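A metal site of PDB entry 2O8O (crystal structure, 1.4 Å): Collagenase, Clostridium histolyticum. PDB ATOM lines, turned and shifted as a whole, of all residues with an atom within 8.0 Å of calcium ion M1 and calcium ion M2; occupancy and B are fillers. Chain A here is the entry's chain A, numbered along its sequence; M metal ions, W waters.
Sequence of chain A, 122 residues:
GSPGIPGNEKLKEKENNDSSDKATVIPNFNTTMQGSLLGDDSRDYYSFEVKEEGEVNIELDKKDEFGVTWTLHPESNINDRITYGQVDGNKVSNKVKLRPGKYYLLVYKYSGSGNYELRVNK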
ATOM      1  N   GLU A  13     -24.617  -0.690 -18.587  1.00  0.00           N
ATOM      2  CA  GLU A  13     -24.476  -0.143 -17.249  1.00  0.00           C
ATOM      3  C   GLU A  13     -23.405  -0.907 -16.521  1.00  0.00           C
ATOM      4  O   GLU A  13     -22.995  -2.006 -16.887  1.00  0.00           O
ATOM      5  CB  GLU A  13     -25.785  -0.265 -16.446  1.00  0.00           C
ATOM      6  CG  GLU A  13     -26.238  -1.700 -16.317  1.00  0.00           C
ATOM      7  CD  GLU A  13     -27.417  -1.862 -15.378  1.00  0.00           C
ATOM      8  OE1 GLU A  13     -27.393  -1.176 -14.337  1.00  0.00           O
ATOM      9  OE2 GLU A  13     -28.170  -2.833 -15.602  1.00  0.00           O
ATOM     10  N   LYS A  14     -22.875  -0.509 -15.440  1.00  0.00           N
ATOM     11  CA  LYS A  14     -21.815  -0.895 -14.547  1.00  0.00           C
ATOM     12  C   LYS A  14     -22.342  -0.904 -13.109  1.00  0.00           C
ATOM     13  O   LYS A  14     -22.436   0.068 -12.378  1.00  0.00           O
ATOM     14  CB  LYS A  14     -20.563  -0.014 -14.676  1.00  0.00           C
ATOM     15  CG  LYS A  14     -19.541   0.057 -15.769  1.00  0.00           C
ATOM     16  CD  LYS A  14     -19.922  -0.296 -17.190  1.00  0.00           C
ATOM     17  CE  LYS A  14     -19.049  -1.367 -17.839  1.00  0.00           C
ATOM     18  NZ  LYS A  14     -19.902  -2.391 -18.521  1.00  0.00           N
ATOM     19  N   GLU A  15     -22.718  -2.116 -12.667  1.00  0.00           N
ATOM     20  CA  GLU A  15     -23.115  -2.284 -11.269  1.00  0.00           C
ATOM     21  C   GLU A  15     -21.869  -2.344 -10.404  1.00  0.00           C
ATOM     22  O   GLU A  15     -20.788  -2.763 -10.893  1.00  0.00           O
ATOM     23  CB  GLU A  15     -23.907  -3.549 -10.988  1.00  0.00           C
ATOM     24  CG  GLU A  15     -25.280  -3.598 -11.662  1.00  0.00           C
ATOM     25  CD  GLU A  15     -26.333  -2.715 -11.007  1.00  0.00           C
ATOM     26  OE1 GLU A  15     -26.133  -2.241  -9.869  1.00  0.00           O
ATOM     27  OE2 GLU A  15     -27.414  -2.590 -11.620  1.00  0.00           O
ATOM     28  N   ASN A  16     -22.018  -1.953  -9.168  1.00  0.00           N
ATOM     29  CA  ASN A  16     -23.175  -1.393  -8.479  1.00  0.00           C
ATOM     30  C   ASN A  16     -23.320   0.094  -8.791  1.00  0.00           C
ATOM     31  O   ASN A  16     -22.351   0.831  -8.630  1.00  0.00           O
ATOM     32  CB  ASN A  16     -22.958  -1.622  -6.985  1.00  0.00           C
ATOM     33  CG  ASN A  16     -24.041  -1.141  -6.077  1.00  0.00           C
ATOM     34  OD1 ASN A  16     -24.555  -0.049  -6.257  1.00  0.00           O
ATOM     35  ND2 ASN A  16     -24.431  -1.919  -5.074  1.00  0.00           N
ATOM     36  N   ASN A  17     -24.511   0.448  -9.215  1.00  0.00           N
ATOM     37  CA  ASN A  17     -24.846   1.809  -9.557  1.00  0.00           C
ATOM     38  C   ASN A  17     -26.113   2.274  -8.847  1.00  0.00           C
ATOM     39  O   ASN A  17     -26.907   3.047  -9.337  1.00  0.00           O
ATOM     40  CB  ASN A  17     -25.031   1.997 -11.063  1.00  0.00           C
ATOM     41  CG  ASN A  17     -26.076   1.060 -11.633  1.00  0.00           C
ATOM     42  OD1 ASN A  17     -26.837   0.467 -10.859  1.00  0.00           O
ATOM     43  ND2 ASN A  17     -26.075   0.917 -12.948  1.00  0.00           N
ATOM     44  N   ASP A  18     -26.249   1.857  -7.599  1.00  0.00           N
ATOM     45  CA  ASP A  18     -27.498   2.097  -6.854  1.00  0.00           C
ATOM     46  C   ASP A  18     -27.600   3.448  -6.143  1.00  0.00           C
ATOM     47  O   ASP A  18     -28.606   3.751  -5.510  1.00  0.00           O
ATOM     48  CB  ASP A  18     -27.673   0.924  -5.887  1.00  0.00           C
ATOM     49  CG  ASP A  18     -27.897  -0.430  -6.557  1.00  0.00           C
ATOM     50  OD1 ASP A  18     -28.023  -1.419  -5.799  1.00  0.00           O
ATOM     51  OD2 ASP A  18     -27.941  -0.608  -7.796  1.00  0.00           O
ATOM     52  N   SER A  19     -26.581   4.280  -6.236  1.00  0.00           N
ATOM     53  CA  SER A  19     -26.558   5.609  -5.636  1.00  0.00           C
ATOM     54  C   SER A  19     -25.869   6.547  -6.609  1.00  0.00           C
ATOM     55  O   SER A  19     -25.162   6.064  -7.452  1.00  0.00           O
ATOM     56  CB  SER A  19     -25.866   5.536  -4.285  1.00  0.00           C
ATOM     57  OG  SER A  19     -24.512   5.151  -4.492  1.00  0.00           O
ATOM     58  N   LYS A  22     -22.227   6.378  -7.329  1.00  0.00           N
ATOM     59  CA  LYS A  22     -21.800   5.244  -8.125  1.00  0.00           C
ATOM     60  C   LYS A  22     -22.486   5.193  -9.481  1.00  0.00           C
ATOM     61  O   LYS A  22     -22.566   4.157 -10.151  1.00  0.00           O
ATOM     62  CB  LYS A  22     -22.168   3.964  -7.371  1.00  0.00           C
ATOM     63  CG  LYS A  22     -21.504   3.901  -5.983  1.00  0.00           C
ATOM     64  CD  LYS A  22     -22.022   2.728  -5.193  1.00  0.00           C
ATOM     65  CE  LYS A  22     -23.530   2.619  -5.104  1.00  0.00           C
ATOM     66  NZ  LYS A  22     -24.165   2.300  -3.822  1.00  0.00           N
ATOM     67  N   THR A  24     -23.504   5.300 -13.317  1.00  0.00           N
ATOM     68  CA  THR A  24     -22.888   4.946 -14.558  1.00  0.00           C
ATOM     69  C   THR A  24     -22.908   6.161 -15.482  1.00  0.00           C
ATOM     70  O   THR A  24     -23.968   6.737 -15.774  1.00  0.00           O
ATOM     71  CB  THR A  24     -23.651   3.821 -15.280  1.00  0.00           C
ATOM     72  OG1 THR A  24     -23.667   2.738 -14.364  1.00  0.00           O
ATOM     73  CG2 THR A  24     -22.999   3.460 -16.601  1.00  0.00           C
ATOM     74  N   GLN A  34     -27.518  -0.212 -22.384  1.00  0.00           N
ATOM     75  CA  GLN A  34     -28.261  -1.408 -22.012  1.00  0.00           C
ATOM     76  C   GLN A  34     -28.255  -1.626 -20.498  1.00  0.00           C
ATOM     77  O   GLN A  34     -27.198  -1.506 -19.896  1.00  0.00           O
ATOM     78  CB  GLN A  34     -27.633  -2.631 -22.685  1.00  0.00           C
ATOM     79  CG  GLN A  34     -27.761  -2.561 -24.211  1.00  0.00           C
ATOM     80  CD  GLN A  34     -27.578  -3.929 -24.848  1.00  0.00           C
ATOM     81  OE1 GLN A  34     -28.164  -4.254 -25.899  1.00  0.00           O
ATOM     82  NE2 GLN A  34     -26.764  -4.736 -24.190  1.00  0.00           N
ATOM     83  N   GLY A  35     -29.404  -1.927 -19.909  1.00  0.00           N
ATOM     84  CA  GLY A  35     -29.414  -2.255 -18.498  1.00  0.00           C
ATOM     85  C   GLY A  35     -30.537  -3.245 -18.190  1.00  0.00           C
ATOM     86  O   GLY A  35     -31.358  -3.615 -19.028  1.00  0.00           O
ATOM     87  N   SER A  36     -30.513  -3.632 -16.921  1.00  0.00           N
ATOM     88  CA  SER A  36     -31.528  -4.526 -16.400  1.00  0.00           C
ATOM     89  C   SER A  36     -31.852  -4.186 -14.946  1.00  0.00           C
ATOM     90  O   SER A  36     -30.961  -3.692 -14.261  1.00  0.00           O
ATOM     91  CB  SER A  36     -31.079  -5.989 -16.533  1.00  0.00           C
ATOM     92  OG  SER A  36     -30.088  -6.322 -15.590  1.00  0.00           O
ATOM     93  N   LEU A  37     -33.084  -4.460 -14.544  1.00  0.00           N
ATOM     94  CA  LEU A  37     -33.572  -4.309 -13.190  1.00  0.00           C
ATOM     95  C   LEU A  37     -34.314  -5.599 -12.820  1.00  0.00           C
ATOM     96  O   LEU A  37     -35.532  -5.676 -12.775  1.00  0.00           O
ATOM     97  CB  LEU A  37     -34.513  -3.119 -13.025  1.00  0.00           C
ATOM     98  CG  LEU A  37     -33.847  -1.737 -13.207  1.00  0.00           C
ATOM     99  CD1 LEU A  37     -34.880  -0.645 -13.349  1.00  0.00           C
ATOM    100  CD2 LEU A  37     -32.916  -1.382 -12.067  1.00  0.00           C
ATOM    101  N   LEU A  38     -33.509  -6.624 -12.596  1.00  0.00           N
ATOM    102  CA  LEU A  38     -33.971  -7.981 -12.281  1.00  0.00           C
ATOM    103  C   LEU A  38     -33.920  -8.228 -10.779  1.00  0.00           C
ATOM    104  O   LEU A  38     -32.917  -7.925 -10.157  1.00  0.00           O
ATOM    105  CB  LEU A  38     -33.128  -9.040 -13.000  1.00  0.00           C
ATOM    106  CG  LEU A  38     -32.840  -8.733 -14.475  1.00  0.00           C
ATOM    107  CD1 LEU A  38     -31.805  -9.742 -14.986  1.00  0.00           C
ATOM    108  CD2 LEU A  38     -34.090  -8.746 -15.332  1.00  0.00           C
ATOM    109  N   ASP A  40     -33.845  -8.039  -6.980  1.00  0.00           N
ATOM    110  CA  ASP A  40     -33.637  -6.979  -6.005  1.00  0.00           C
ATOM    111  C   ASP A  40     -32.732  -5.865  -6.538  1.00  0.00           C
ATOM    112  O   ASP A  40     -32.407  -4.946  -5.771  1.00  0.00           O
ATOM    113  CB  ASP A  40     -33.142  -7.524  -4.676  1.00  0.00           C
ATOM    114  CG  ASP A  40     -31.775  -8.142  -4.672  1.00  0.00           C
ATOM    115  OD1 ASP A  40     -30.983  -7.926  -5.590  1.00  0.00           O
ATOM    116  OD2 ASP A  40     -31.559  -8.896  -3.678  1.00  0.00           O
ATOM    117  N   ASP A  41     -32.351  -5.901  -7.807  1.00  0.00           N
ATOM    118  CA  ASP A  41     -31.752  -4.719  -8.412  1.00  0.00           C
ATOM    119  C   ASP A  41     -32.899  -3.826  -8.877  1.00  0.00           C
ATOM    120  O   ASP A  41     -33.486  -4.107  -9.938  1.00  0.00           O
ATOM    121  CB  ASP A  41     -30.831  -5.094  -9.555  1.00  0.00           C
ATOM    122  CG  ASP A  41     -30.162  -3.954 -10.244  1.00  0.00           C
ATOM    123  OD1 ASP A  41     -29.772  -3.007  -9.525  1.00  0.00           O
ATOM    124  OD2 ASP A  41     -30.022  -3.980 -11.486  1.00  0.00           O
ATOM    125  N   SER A  42     -33.213  -2.796  -8.072  1.00  0.00           N
ATOM    126  CA  SER A  42     -34.390  -1.985  -8.374  1.00  0.00           C
ATOM    127  C   SER A  42     -34.074  -0.564  -8.829  1.00  0.00           C
ATOM    128  O   SER A  42     -35.039   0.142  -9.167  1.00  0.00           O
ATOM    129  CB  SER A  42     -35.329  -1.814  -7.180  1.00  0.00           C
ATOM    130  OG  SER A  42     -34.624  -1.626  -6.017  1.00  0.00           O
ATOM    131  N   ARG A  43     -32.817  -0.198  -8.803  1.00  0.00           N
ATOM    132  CA  ARG A  43     -32.339   1.141  -9.121  1.00  0.00           C
ATOM    133  C   ARG A  43     -31.051   1.101  -9.918  1.00  0.00           C
ATOM    134  O   ARG A  43     -30.126   0.387  -9.488  1.00  0.00           O
ATOM    135  CB  ARG A  43     -32.024   1.952  -7.810  1.00  0.00           C
ATOM    136  CG  ARG A  43     -33.192   2.050  -6.875  1.00  0.00           C
ATOM    137  CD  ARG A  43     -32.722   2.448  -5.508  1.00  0.00           C
ATOM    138  NE  ARG A  43     -31.967   3.663  -5.417  1.00  0.00           N
ATOM    139  CZ  ARG A  43     -32.472   4.860  -5.125  1.00  0.00           C
ATOM    140  NH1 ARG A  43     -33.775   5.090  -4.920  1.00  0.00           N
ATOM    141  NH2 ARG A  43     -31.583   5.835  -5.074  1.00  0.00           N
ATOM    142  N   ASP A  44     -30.983   1.864 -11.002  1.00  0.00           N
ATOM    143  CA  ASP A  44     -29.766   2.082 -11.772  1.00  0.00           C
ATOM    144  C   ASP A  44     -29.597   3.588 -11.967  1.00  0.00           C
ATOM    145  O   ASP A  44     -30.407   4.216 -12.649  1.00  0.00           O
ATOM    146  CB  ASP A  44     -29.865   1.390 -13.118  1.00  0.00           C
ATOM    147  CG  ASP A  44     -29.907  -0.111 -13.095  1.00  0.00           C
ATOM    148  OD1 ASP A  44     -29.505  -0.703 -12.074  1.00  0.00           O
ATOM    149  OD2 ASP A  44     -30.344  -0.724 -14.099  1.00  0.00           O
ATOM    150  N   TYR A  45     -28.576   4.131 -11.322  1.00  0.00           N
ATOM    151  CA  TYR A  45     -28.240   5.541 -11.473  1.00  0.00           C
ATOM    152  C   TYR A  45     -27.292   5.764 -12.635  1.00  0.00           C
ATOM    153  O   TYR A  45     -26.305   5.012 -12.772  1.00  0.00           O
ATOM    154  CB  TYR A  45     -27.605   6.126 -10.212  1.00  0.00           C
ATOM    155  CG  TYR A  45     -28.433   7.217  -9.562  1.00  0.00           C
ATOM    156  CD1 TYR A  45     -28.902   7.117  -8.269  1.00  0.00           C
ATOM    157  CD2 TYR A  45     -28.782   8.367 -10.237  1.00  0.00           C
ATOM    158  CE1 TYR A  45     -29.661   8.048  -7.608  1.00  0.00           C
ATOM    159  CE2 TYR A  45     -29.556   9.325  -9.594  1.00  0.00           C
ATOM    160  CZ  TYR A  45     -29.993   9.181  -8.299  1.00  0.00           C
ATOM    161  OH  TYR A  45     -30.752  10.180  -7.730  1.00  0.00           O
ATOM    162  N   TYR A  46     -27.589   6.790 -13.416  1.00  0.00           N
ATOM    163  CA  TYR A  46     -26.728   7.275 -14.487  1.00  0.00           C
ATOM    164  C   TYR A  46     -26.445   8.765 -14.302  1.00  0.00           C
ATOM    165  O   TYR A  46     -27.158   9.448 -13.566  1.00  0.00           O
ATOM    166  CB  TYR A  46     -27.393   7.075 -15.844  1.00  0.00           C
ATOM    167  CG  TYR A  46     -27.707   5.665 -16.190  1.00  0.00           C
ATOM    168  CD1 TYR A  46     -28.866   5.042 -15.782  1.00  0.00           C
ATOM    169  CD2 TYR A  46     -26.823   4.926 -16.942  1.00  0.00           C
ATOM    170  CE1 TYR A  46     -29.151   3.726 -16.120  1.00  0.00           C
ATOM    171  CE2 TYR A  46     -27.065   3.626 -17.301  1.00  0.00           C
ATOM    172  CZ  TYR A  46     -28.227   3.031 -16.875  1.00  0.00           C
ATOM    173  OH  TYR A  46     -28.433   1.710 -17.250  1.00  0.00           O
ATOM    174  N   LEU A 106     -32.030   8.644 -12.477  1.00  0.00           N
ATOM    175  CA  LEU A 106     -32.296   7.459 -11.715  1.00  0.00           C
ATOM    176  C   LEU A 106     -33.364   6.655 -12.492  1.00  0.00           C
ATOM    177  O   LEU A 106     -34.497   7.143 -12.620  1.00  0.00           O
ATOM    178  CB  LEU A 106     -32.803   7.761 -10.311  1.00  0.00           C
ATOM    179  CG  LEU A 106     -33.311   6.543  -9.526  1.00  0.00           C
ATOM    180  CD1 LEU A 106     -32.175   5.587  -9.280  1.00  0.00           C
ATOM    181  CD2 LEU A 106     -33.935   7.047  -8.234  1.00  0.00           C
ATOM    182  N   VAL A 107     -32.981   5.490 -12.942  1.00  0.00           N
ATOM    183  CA  VAL A 107     -33.922   4.520 -13.545  1.00  0.00           C
ATOM    184  C   VAL A 107     -34.308   3.545 -12.447  1.00  0.00           C
ATOM    185  O   VAL A 107     -33.438   2.964 -11.776  1.00  0.00           O
ATOM    186  CB  VAL A 107     -33.306   3.808 -14.758  1.00  0.00           C
ATOM    187  CG1 VAL A 107     -34.260   2.754 -15.277  1.00  0.00           C
ATOM    188  CG2 VAL A 107     -32.906   4.801 -15.847  1.00  0.00           C
ATOM    189  N   GLY A 114     -37.212  -6.629 -15.402  1.00  0.00           N
ATOM    190  CA  GLY A 114     -36.971  -6.672 -16.833  1.00  0.00           C
ATOM    191  C   GLY A 114     -35.702  -5.955 -17.249  1.00  0.00           C
ATOM    192  O   GLY A 114     -35.006  -5.333 -16.433  1.00  0.00           O
ATOM    193  N   TYR A 116     -33.985  -3.194 -20.221  1.00  0.00           N
ATOM    194  CA  TYR A 116     -34.325  -1.954 -20.881  1.00  0.00           C
ATOM    195  C   TYR A 116     -33.130  -1.431 -21.684  1.00  0.00           C
ATOM    196  O   TYR A 116     -31.963  -1.809 -21.495  1.00  0.00           O
ATOM    197  CB  TYR A 116     -34.827  -0.884 -19.862  1.00  0.00           C
ATOM    198  CG  TYR A 116     -33.745  -0.456 -18.889  1.00  0.00           C
ATOM    199  CD1 TYR A 116     -32.893   0.589 -19.122  1.00  0.00           C
ATOM    200  CD2 TYR A 116     -33.546  -1.132 -17.694  1.00  0.00           C
ATOM    201  CE1 TYR A 116     -31.903   0.989 -18.277  1.00  0.00           C
ATOM    202  CE2 TYR A 116     -32.542  -0.766 -16.825  1.00  0.00           C
ATOM    203  CZ  TYR A 116     -31.729   0.300 -17.119  1.00  0.00           C
ATOM    204  OH  TYR A 116     -30.744   0.671 -16.263  1.00  0.00           O
HETATM  205 CA    CA M   1     -28.388  -1.080 -10.030  1.00  0.00          CA
HETATM  206 CA    CA M   2     -29.014  -2.808 -13.309  1.00  0.00          CA
HETATM  207  O   HOH W   1     -28.024  -4.995 -13.680  1.00  0.00           O
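Five residues have an atom within 4 Å of calcium ion M2: Glu 13, Glu 15, Ser 36, Asp 41 and Asp 44.
The backbone NH of Asp 18 is in hydrogen-bond range of the side-chain amide oxygen of Asn 16, 2.9 Å away.
ND2 of Asn 17 sits close to OE1 of Glu 13, at 2.8 Å.
The backbone carbonyl oxygen (O) of Asn 17 is in hydrogen-bond range of the backbone NH (N) of Tyr 45 (2.8 Å).
The side-chain amide nitrogen of Asn 17 lies within hydrogen-bond range of the side-chain hydroxyl of Thr 24, 3.3 Å away.
The side-chain hydroxyl of Tyr 116 lies close to the side-chain carboxylate of Asp 44 (2.6 Å).
N of Asp 44 lies within hydrogen-bond range of O of Val 107 (2.8 Å).
The backbone NH of Glu 13 is in hydrogen-bond range of the backbone carbonyl oxygen of Gln 34, 3.0 Å away.
Calcium ion M2 is bound by OE2 of Glu 15 (2.3 Å), O of Ser 36 (2.3 Å), OD2 of Asp 41 (2.4 Å), water W1 (2.4 Å), OE2 of Glu 13 (2.4 Å), OD1 of Asp 44 (2.5 Å), OE1 of Glu 13 (2.5 Å) and OD2 of Asp 44 (2.6 Å).
Calcium ion M1 is bound by OD2 of Asp 18, O of Arg 43, OD1 of Asn 17, OD1 of Asp 44, OE2 of Glu 15, OD1 of Asp 41 and OE1 of Glu 15.
Calcium ion M1 has seven donor atoms within binding distance.
Six residues have an atom within 4 Å of calcium ion M1: Glu 15, Asn 17, Asp 18, Asp 41, Arg 43 and Asp 44.
The nearest printed residue that does not touch calcium ion M1 is Glu 13 (4.4 Å).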
